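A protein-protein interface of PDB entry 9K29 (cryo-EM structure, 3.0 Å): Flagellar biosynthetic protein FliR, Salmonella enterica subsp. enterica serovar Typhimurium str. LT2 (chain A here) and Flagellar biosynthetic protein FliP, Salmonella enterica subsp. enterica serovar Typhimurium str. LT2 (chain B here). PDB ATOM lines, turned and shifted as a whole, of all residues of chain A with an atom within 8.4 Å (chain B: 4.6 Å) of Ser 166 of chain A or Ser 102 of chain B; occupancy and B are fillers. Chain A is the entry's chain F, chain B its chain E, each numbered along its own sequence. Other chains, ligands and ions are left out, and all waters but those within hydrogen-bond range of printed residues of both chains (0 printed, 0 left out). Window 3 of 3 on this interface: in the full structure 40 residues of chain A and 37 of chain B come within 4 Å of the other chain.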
ATOM      1  N   TRP A  72     -34.326  27.603   8.311  1.00  0.00           N
ATOM      2  CA  TRP A  72     -33.303  27.033   7.439  1.00  0.00           C
ATOM      3  C   TRP A  72     -33.927  26.345   6.230  1.00  0.00           C
ATOM      4  O   TRP A  72     -33.475  26.534   5.095  1.00  0.00           O
ATOM      5  CB  TRP A  72     -32.423  26.058   8.221  1.00  0.00           C
ATOM      6  CG  TRP A  72     -31.262  26.722   8.895  1.00  0.00           C
ATOM      7  CD1 TRP A  72     -31.222  27.205  10.170  1.00  0.00           C
ATOM      8  CD2 TRP A  72     -29.968  26.972   8.330  1.00  0.00           C
ATOM      9  NE1 TRP A  72     -29.988  27.746  10.433  1.00  0.00           N
ATOM     10  CE2 TRP A  72     -29.199  27.613   9.320  1.00  0.00           C
ATOM     11  CE3 TRP A  72     -29.386  26.717   7.084  1.00  0.00           C
ATOM     12  CZ2 TRP A  72     -27.878  28.005   9.104  1.00  0.00           C
ATOM     13  CZ3 TRP A  72     -28.074  27.107   6.872  1.00  0.00           C
ATOM     14  CH2 TRP A  72     -27.336  27.743   7.876  1.00  0.00           C
ATOM     15  N   LEU A  79     -34.461  29.721  -1.993  1.00  0.00           N
ATOM     16  CA  LEU A  79     -33.314  29.718  -2.896  1.00  0.00           C
ATOM     17  C   LEU A  79     -33.611  28.941  -4.171  1.00  0.00           C
ATOM     18  O   LEU A  79     -33.349  29.427  -5.276  1.00  0.00           O
ATOM     19  CB  LEU A  79     -32.081  29.151  -2.188  1.00  0.00           C
ATOM     20  CG  LEU A  79     -31.137  30.109  -1.455  1.00  0.00           C
ATOM     21  CD1 LEU A  79     -30.474  30.960  -2.497  1.00  0.00           C
ATOM     22  CD2 LEU A  79     -31.828  31.017  -0.462  1.00  0.00           C
ATOM     23  N   PRO A 163     -27.131  21.691   2.623  1.00  0.00           N
ATOM     24  CA  PRO A 163     -26.972  22.982   1.945  1.00  0.00           C
ATOM     25  C   PRO A 163     -26.903  22.819   0.435  1.00  0.00           C
ATOM     26  O   PRO A 163     -26.406  21.817  -0.085  1.00  0.00           O
ATOM     27  CB  PRO A 163     -25.648  23.519   2.506  1.00  0.00           C
ATOM     28  CG  PRO A 163     -25.428  22.757   3.777  1.00  0.00           C
ATOM     29  CD  PRO A 163     -26.006  21.399   3.525  1.00  0.00           C
ATOM     30  N   VAL A 164     -27.414  23.823  -0.267  1.00  0.00           N
ATOM     31  CA  VAL A 164     -27.379  23.831  -1.725  1.00  0.00           C
ATOM     32  C   VAL A 164     -26.008  24.296  -2.194  1.00  0.00           C
ATOM     33  O   VAL A 164     -25.409  25.210  -1.614  1.00  0.00           O
ATOM     34  CB  VAL A 164     -28.508  24.716  -2.287  1.00  0.00           C
ATOM     35  CG1 VAL A 164     -28.349  26.159  -1.831  1.00  0.00           C
ATOM     36  CG2 VAL A 164     -28.549  24.633  -3.806  1.00  0.00           C
ATOM     37  N   ASN A 165     -25.490  23.646  -3.233  1.00  0.00           N
ATOM     38  CA  ASN A 165     -24.201  24.031  -3.787  1.00  0.00           C
ATOM     39  C   ASN A 165     -24.280  25.420  -4.407  1.00  0.00           C
ATOM     40  O   ASN A 165     -25.246  25.766  -5.091  1.00  0.00           O
ATOM     41  CB  ASN A 165     -23.742  23.013  -4.830  1.00  0.00           C
ATOM     42  CG  ASN A 165     -22.443  23.409  -5.500  1.00  0.00           C
ATOM     43  OD1 ASN A 165     -22.363  23.493  -6.725  1.00  0.00           O
ATOM     44  ND2 ASN A 165     -21.416  23.660  -4.697  1.00  0.00           N
ATOM     45  N   SER A 166     -23.243  26.221  -4.164  1.00  0.00           N
ATOM     46  CA  SER A 166     -23.215  27.604  -4.614  1.00  0.00           C
ATOM     47  C   SER A 166     -22.489  27.805  -5.934  1.00  0.00           C
ATOM     48  O   SER A 166     -22.576  28.898  -6.504  1.00  0.00           O
ATOM     49  CB  SER A 166     -22.565  28.495  -3.548  1.00  0.00           C
ATOM     50  OG  SER A 166     -21.201  28.156  -3.368  1.00  0.00           O
ATOM     51  N   ASN A 167     -21.772  26.796  -6.430  1.00  0.00           N
ATOM     52  CA  ASN A 167     -21.145  26.922  -7.742  1.00  0.00           C
ATOM     53  C   ASN A 167     -22.196  27.068  -8.833  1.00  0.00           C
ATOM     54  O   ASN A 167     -21.988  27.790  -9.815  1.00  0.00           O
ATOM     55  CB  ASN A 167     -20.246  25.717  -8.013  1.00  0.00           C
ATOM     56  CG  ASN A 167     -18.967  25.752  -7.204  1.00  0.00           C
ATOM     57  OD1 ASN A 167     -18.654  26.753  -6.560  1.00  0.00           O
ATOM     58  ND2 ASN A 167     -18.216  24.657  -7.233  1.00  0.00           N
ATOM     59  N   ALA A 168     -23.334  26.390  -8.675  1.00  0.00           N
ATOM     60  CA  ALA A 168     -24.425  26.532  -9.632  1.00  0.00           C
ATOM     61  C   ALA A 168     -24.977  27.952  -9.632  1.00  0.00           C
ATOM     62  O   ALA A 168     -25.298  28.501 -10.693  1.00  0.00           O
ATOM     63  CB  ALA A 168     -25.530  25.526  -9.317  1.00  0.00           C
ATOM     64  N   PHE A 169     -25.104  28.558  -8.449  1.00  0.00           N
ATOM     65  CA  PHE A 169     -25.585  29.933  -8.370  1.00  0.00           C
ATOM     66  C   PHE A 169     -24.640  30.887  -9.085  1.00  0.00           C
ATOM     67  O   PHE A 169     -25.082  31.775  -9.823  1.00  0.00           O
ATOM     68  CB  PHE A 169     -25.755  30.347  -6.910  1.00  0.00           C
ATOM     69  CG  PHE A 169     -27.028  29.859  -6.289  1.00  0.00           C
ATOM     70  CD1 PHE A 169     -28.249  30.356  -6.706  1.00  0.00           C
ATOM     71  CD2 PHE A 169     -27.004  28.898  -5.294  1.00  0.00           C
ATOM     72  CE1 PHE A 169     -29.424  29.908  -6.139  1.00  0.00           C
ATOM     73  CE2 PHE A 169     -28.176  28.444  -4.724  1.00  0.00           C
ATOM     74  CZ  PHE A 169     -29.388  28.949  -5.149  1.00  0.00           C
ATOM     75  N   MET A 170     -23.332  30.714  -8.886  1.00  0.00           N
ATOM     76  CA  MET A 170     -22.371  31.565  -9.577  1.00  0.00           C
ATOM     77  C   MET A 170     -22.417  31.331 -11.079  1.00  0.00           C
ATOM     78  O   MET A 170     -22.301  32.275 -11.864  1.00  0.00           O
ATOM     79  CB  MET A 170     -20.962  31.318  -9.046  1.00  0.00           C
ATOM     80  CG  MET A 170     -19.890  32.106  -9.775  1.00  0.00           C
ATOM     81  SD  MET A 170     -20.268  33.870  -9.748  1.00  0.00           S
ATOM     82  CE  MET A 170     -18.942  34.531 -10.747  1.00  0.00           C
ATOM     83  N   ALA A 171     -22.578  30.073 -11.497  1.00  0.00           N
ATOM     84  CA  ALA A 171     -22.658  29.772 -12.921  1.00  0.00           C
ATOM     85  C   ALA A 171     -23.870  30.425 -13.569  1.00  0.00           C
ATOM     86  O   ALA A 171     -23.758  30.985 -14.665  1.00  0.00           O
ATOM     87  CB  ALA A 171     -22.691  28.260 -13.141  1.00  0.00           C
ATOM     88  N   LEU A 172     -25.029  30.376 -12.913  1.00  0.00           N
ATOM     89  CA  LEU A 172     -26.224  30.987 -13.480  1.00  0.00           C
ATOM     90  C   LEU A 172     -26.246  32.503 -13.331  1.00  0.00           C
ATOM     91  O   LEU A 172     -26.971  33.171 -14.077  1.00  0.00           O
ATOM     92  CB  LEU A 172     -27.486  30.372 -12.862  1.00  0.00           C
ATOM     93  CG  LEU A 172     -27.749  30.435 -11.358  1.00  0.00           C
ATOM     94  CD1 LEU A 172     -28.475  31.703 -10.983  1.00  0.00           C
ATOM     95  CD2 LEU A 172     -28.542  29.219 -10.912  1.00  0.00           C
ATOM     96  N   ALA A 173     -25.476  33.064 -12.395  1.00  0.00           N
ATOM     97  CA  ALA A 173     -25.293  34.511 -12.371  1.00  0.00           C
ATOM     98  C   ALA A 173     -24.365  34.962 -13.491  1.00  0.00           C
ATOM     99  O   ALA A 173     -24.621  35.978 -14.147  1.00  0.00           O
ATOM    100  CB  ALA A 173     -24.746  34.953 -11.014  1.00  0.00           C
ATOM    101  N   ILE A 254     -27.799  23.158 -14.728  1.00  0.00           N
ATOM    102  CA  ILE A 254     -27.529  23.718 -13.407  1.00  0.00           C
ATOM    103  C   ILE A 254     -28.217  22.896 -12.323  1.00  0.00           C
ATOM    104  O   ILE A 254     -27.629  22.610 -11.272  1.00  0.00           O
ATOM    105  CB  ILE A 254     -27.951  25.197 -13.362  1.00  0.00           C
ATOM    106  CG1 ILE A 254     -26.983  26.044 -14.188  1.00  0.00           C
ATOM    107  CG2 ILE A 254     -28.004  25.699 -11.936  1.00  0.00           C
ATOM    108  CD1 ILE A 254     -27.591  27.315 -14.721  1.00  0.00           C
ATOM    109  N   GLU A 257     -26.414  19.855 -11.704  1.00  0.00           N
ATOM    110  CA  GLU A 257     -25.154  20.133 -11.028  1.00  0.00           C
ATOM    111  C   GLU A 257     -25.305  20.534  -9.567  1.00  0.00           C
ATOM    112  O   GLU A 257     -24.330  20.448  -8.819  1.00  0.00           O
ATOM    113  CB  GLU A 257     -24.392  21.243 -11.764  1.00  0.00           C
ATOM    114  CG  GLU A 257     -23.644  20.774 -13.000  1.00  0.00           C
ATOM    115  CD  GLU A 257     -22.997  21.916 -13.756  1.00  0.00           C
ATOM    116  OE1 GLU A 257     -22.802  22.994 -13.155  1.00  0.00           O
ATOM    117  OE2 GLU A 257     -22.683  21.738 -14.952  1.00  0.00           O
ATOM    118  N   MET A 258     -26.492  20.977  -9.146  1.00  0.00           N
ATOM    119  CA  MET A 258     -26.671  21.400  -7.756  1.00  0.00           C
ATOM    120  C   MET A 258     -26.441  20.297  -6.728  1.00  0.00           C
ATOM    121  O   MET A 258     -25.653  20.519  -5.790  1.00  0.00           O
ATOM    122  CB  MET A 258     -28.066  22.004  -7.565  1.00  0.00           C
ATOM    123  CG  MET A 258     -28.315  23.318  -8.280  1.00  0.00           C
ATOM    124  SD  MET A 258     -29.993  23.907  -7.973  1.00  0.00           S
ATOM    125  CE  MET A 258     -30.042  25.380  -8.988  1.00  0.00           C
ATOM    126  N   ASN A 261     -22.887  18.499  -4.637  1.00  0.00           N
ATOM    127  CA  ASN A 261     -22.025  19.123  -3.641  1.00  0.00           C
ATOM    128  C   ASN A 261     -22.799  19.657  -2.437  1.00  0.00           C
ATOM    129  O   ASN A 261     -22.521  20.766  -1.972  1.00  0.00           O
ATOM    130  CB  ASN A 261     -21.208  20.244  -4.287  1.00  0.00           C
ATOM    131  CG  ASN A 261     -19.989  20.629  -3.465  1.00  0.00           C
ATOM    132  OD1 ASN A 261     -19.737  20.061  -2.402  1.00  0.00           O
ATOM    133  ND2 ASN A 261     -19.228  21.601  -3.956  1.00  0.00           N
ATOM    134  N   ASN A 262     -23.767  18.901  -1.930  1.00  0.00           N
ATOM    135  CA  ASN A 262     -24.468  19.305  -0.716  1.00  0.00           C
ATOM    136  C   ASN A 262     -23.601  19.066   0.516  1.00  0.00           C
ATOM    137  O   ASN A 262     -22.934  18.037   0.628  1.00  0.00           O
ATOM    138  CB  ASN A 262     -25.797  18.559  -0.572  1.00  0.00           C
ATOM    139  CG  ASN A 262     -26.804  18.950  -1.634  1.00  0.00           C
ATOM    140  OD1 ASN A 262     -27.209  18.128  -2.452  1.00  0.00           O
ATOM    141  ND2 ASN A 262     -27.212  20.215  -1.627  1.00  0.00           N
ATOM    142  N   PHE B  98     -25.425  35.109  -2.819  1.00  0.00           N
ATOM    143  CA  PHE B  98     -25.552  33.736  -2.341  1.00  0.00           C
ATOM    144  C   PHE B  98     -24.289  32.932  -2.619  1.00  0.00           C
ATOM    145  O   PHE B  98     -23.879  32.103  -1.799  1.00  0.00           O
ATOM    146  CB  PHE B  98     -26.777  33.078  -2.974  1.00  0.00           C
ATOM    147  CG  PHE B  98     -28.075  33.730  -2.592  1.00  0.00           C
ATOM    148  CD1 PHE B  98     -28.249  34.256  -1.322  1.00  0.00           C
ATOM    149  CD2 PHE B  98     -29.114  33.832  -3.501  1.00  0.00           C
ATOM    150  CE1 PHE B  98     -29.436  34.861  -0.963  1.00  0.00           C
ATOM    151  CE2 PHE B  98     -30.305  34.437  -3.147  1.00  0.00           C
ATOM    152  CZ  PHE B  98     -30.465  34.950  -1.875  1.00  0.00           C
ATOM    153  N   PHE B  99     -23.659  33.154  -3.775  1.00  0.00           N
ATOM    154  CA  PHE B  99     -22.417  32.448  -4.073  1.00  0.00           C
ATOM    155  C   PHE B  99     -21.256  32.982  -3.244  1.00  0.00           C
ATOM    156  O   PHE B  99     -20.459  32.207  -2.702  1.00  0.00           O
ATOM    157  CB  PHE B  99     -22.090  32.554  -5.560  1.00  0.00           C
ATOM    158  CG  PHE B  99     -20.635  32.352  -5.870  1.00  0.00           C
ATOM    159  CD1 PHE B  99     -20.055  31.100  -5.752  1.00  0.00           C
ATOM    160  CD2 PHE B  99     -19.847  33.414  -6.283  1.00  0.00           C
ATOM    161  CE1 PHE B  99     -18.718  30.911  -6.040  1.00  0.00           C
ATOM    162  CE2 PHE B  99     -18.508  33.230  -6.571  1.00  0.00           C
ATOM    163  CZ  PHE B  99     -17.943  31.978  -6.449  1.00  0.00           C
ATOM    164  N   ILE B 100     -21.139  34.306  -3.143  1.00  0.00           N
ATOM    165  CA  ILE B 100     -19.991  34.921  -2.490  1.00  0.00           C
ATOM    166  C   ILE B 100     -19.959  34.579  -1.008  1.00  0.00           C
ATOM    167  O   ILE B 100     -18.906  34.232  -0.460  1.00  0.00           O
ATOM    168  CB  ILE B 100     -20.013  36.443  -2.722  1.00  0.00           C
ATOM    169  CG1 ILE B 100     -19.469  36.780  -4.111  1.00  0.00           C
ATOM    170  CG2 ILE B 100     -19.234  37.160  -1.647  1.00  0.00           C
ATOM    171  CD1 ILE B 100     -19.613  38.236  -4.483  1.00  0.00           C
ATOM    172  N   MET B 101     -21.102  34.666  -0.336  1.00  0.00           N
ATOM    173  CA  MET B 101     -21.151  34.399   1.093  1.00  0.00           C
ATOM    174  C   MET B 101     -21.526  32.965   1.424  1.00  0.00           C
ATOM    175  O   MET B 101     -21.936  32.698   2.558  1.00  0.00           O
ATOM    176  CB  MET B 101     -22.126  35.353   1.783  1.00  0.00           C
ATOM    177  CG  MET B 101     -21.674  36.795   1.763  1.00  0.00           C
ATOM    178  SD  MET B 101     -22.885  37.889   2.511  1.00  0.00           S
ATOM    179  CE  MET B 101     -22.736  37.420   4.231  1.00  0.00           C
ATOM    180  N   SER B 102     -21.406  32.050   0.472  1.00  0.00           N
ATOM    181  CA  SER B 102     -21.587  30.635   0.763  1.00  0.00           C
ATOM    182  C   SER B 102     -20.613  30.147   1.834  1.00  0.00           C
ATOM    183  O   SER B 102     -21.021  29.349   2.685  1.00  0.00           O
ATOM    184  CB  SER B 102     -21.474  29.793  -0.513  1.00  0.00           C
ATOM    185  OG  SER B 102     -20.179  29.817  -1.081  1.00  0.00           O
ATOM    186  N   PRO B 103     -19.330  30.556   1.841  1.00  0.00           N
ATOM    187  CA  PRO B 103     -18.482  30.161   2.980  1.00  0.00           C
ATOM    188  C   PRO B 103     -18.988  30.681   4.312  1.00  0.00           C
ATOM    189  O   PRO B 103     -18.889  29.976   5.321  1.00  0.00           O
ATOM    190  CB  PRO B 103     -17.111  30.750   2.618  1.00  0.00           C
ATOM    191  CG  PRO B 103     -17.407  31.845   1.677  1.00  0.00           C
ATOM    192  CD  PRO B 103     -18.555  31.348   0.868  1.00  0.00           C
ATOM    193  N   VAL B 104     -19.496  31.917   4.321  1.00  0.00           N
ATOM    194  CA  VAL B 104     -19.984  32.540   5.587  1.00  0.00           C
ATOM    195  C   VAL B 104     -21.135  31.691   6.135  1.00  0.00           C
ATOM    196  O   VAL B 104     -21.067  31.294   7.315  1.00  0.00           O
ATOM    197  CB  VAL B 104     -20.426  33.998   5.362  1.00  0.00           C
ATOM    198  CG1 VAL B 104     -20.940  34.636   6.643  1.00  0.00           C
ATOM    199  CG2 VAL B 104     -19.315  34.839   4.752  1.00  0.00           C
ATOM    200  N   ILE B 105     -22.145  31.425   5.302  1.00  0.00           N
ATOM    201  CA  ILE B 105     -23.328  30.632   5.749  1.00  0.00           C
ATOM    202  C   ILE B 105     -22.854  29.236   6.165  1.00  0.00           C
ATOM    203  O   ILE B 105     -23.347  28.727   7.190  1.00  0.00           O
ATOM    204  CB  ILE B 105     -24.390  30.568   4.635  1.00  0.00           C
ATOM    205  CG1 ILE B 105     -24.691  31.955   4.063  1.00  0.00           C
ATOM    206  CG2 ILE B 105     -25.650  29.874   5.129  1.00  0.00           C
ATOM    207  CD1 ILE B 105     -25.127  32.963   5.101  1.00  0.00           C
ATOM    208  N   ASP B 106     -21.929  28.651   5.399  1.00  0.00           N
ATOM    209  CA  ASP B 106     -21.401  27.301   5.729  1.00  0.00           C
ATOM    210  C   ASP B 106     -20.815  27.339   7.142  1.00  0.00           C
ATOM    211  O   ASP B 106     -21.184  26.473   7.959  1.00  0.00           O
ATOM    212  CB  ASP B 106     -20.365  26.840   4.702  1.00  0.00           C
ATOM    213  CG  ASP B 106     -19.838  25.440   4.962  1.00  0.00           C
ATOM    214  OD1 ASP B 106     -20.442  24.729   5.790  1.00  0.00           O
ATOM    215  OD2 ASP B 106     -18.824  25.073   4.337  1.00  0.00           O
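The side-chain hydroxyl of Ser 166 of chain A lies within hydrogen-bond range of the side-chain hydroxyl of Ser 102 of chain B, at 3.0 Å.
OG of Ser 102 of chain B sits at hydrogen-bond distance from O of Phe 99 of chain B (2.9 Å).
Among the printed residues, merely in contact across the chains: Trp 72 of chain A with Ile 105 of chain B (3.9 Å), Leu 79 of chain A with Phe 98 of chain B (3.3 Å), Ser 166 of chain A with Phe 99 of chain B (3.4 Å) and Met 170 of chain A with Phe 99 of chain B (3.4 Å).
Of the printed residues of chain B, Trp 72 of chain A touches Ile 105. Of the printed residues of chain B, Leu 79 of chain A touches Phe 98 (3.3 Å). Pro 163 of chain A touches none of the printed residues of chain B. Ser 166 of chain A touches just these residues of chain B: Phe 99 (3.4 Å) and Ser 102 (3.0 Å). Of the printed residues of chain B, Met 170 of chain A touches Phe 99 (3.4 Å). Ala 171 of chain A touches none of the printed residues of chain B. Printed residues of chain A within 4 Å of Phe 98 of chain B: Leu 79 (3.3 Å). Printed residues of chain A within 4 Å of Phe 99 of chain B: Ser 166 (3.4 Å) and Met 170 (3.4 Å). Ser 102 of chain B touches just one residue of chain A: Ser 166 (3.0 Å). The nearest residue of chain B that does not touch Ser 166 of chain A is Phe 98 of chain B (4.2 Å). The nearest residue of chain A that does not touch Ser 102 of chain B is Val 164 of chain A (6.1 Å). The nearest printed residue of chain B that does not touch Leu 79 of chain A is Phe 99 of chain B (7.3 Å).
Hydrophobic or aromatic side chains of chain B within 4 Å of the printed part of chain A: Phe 98, Phe 99 and Ile 105.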
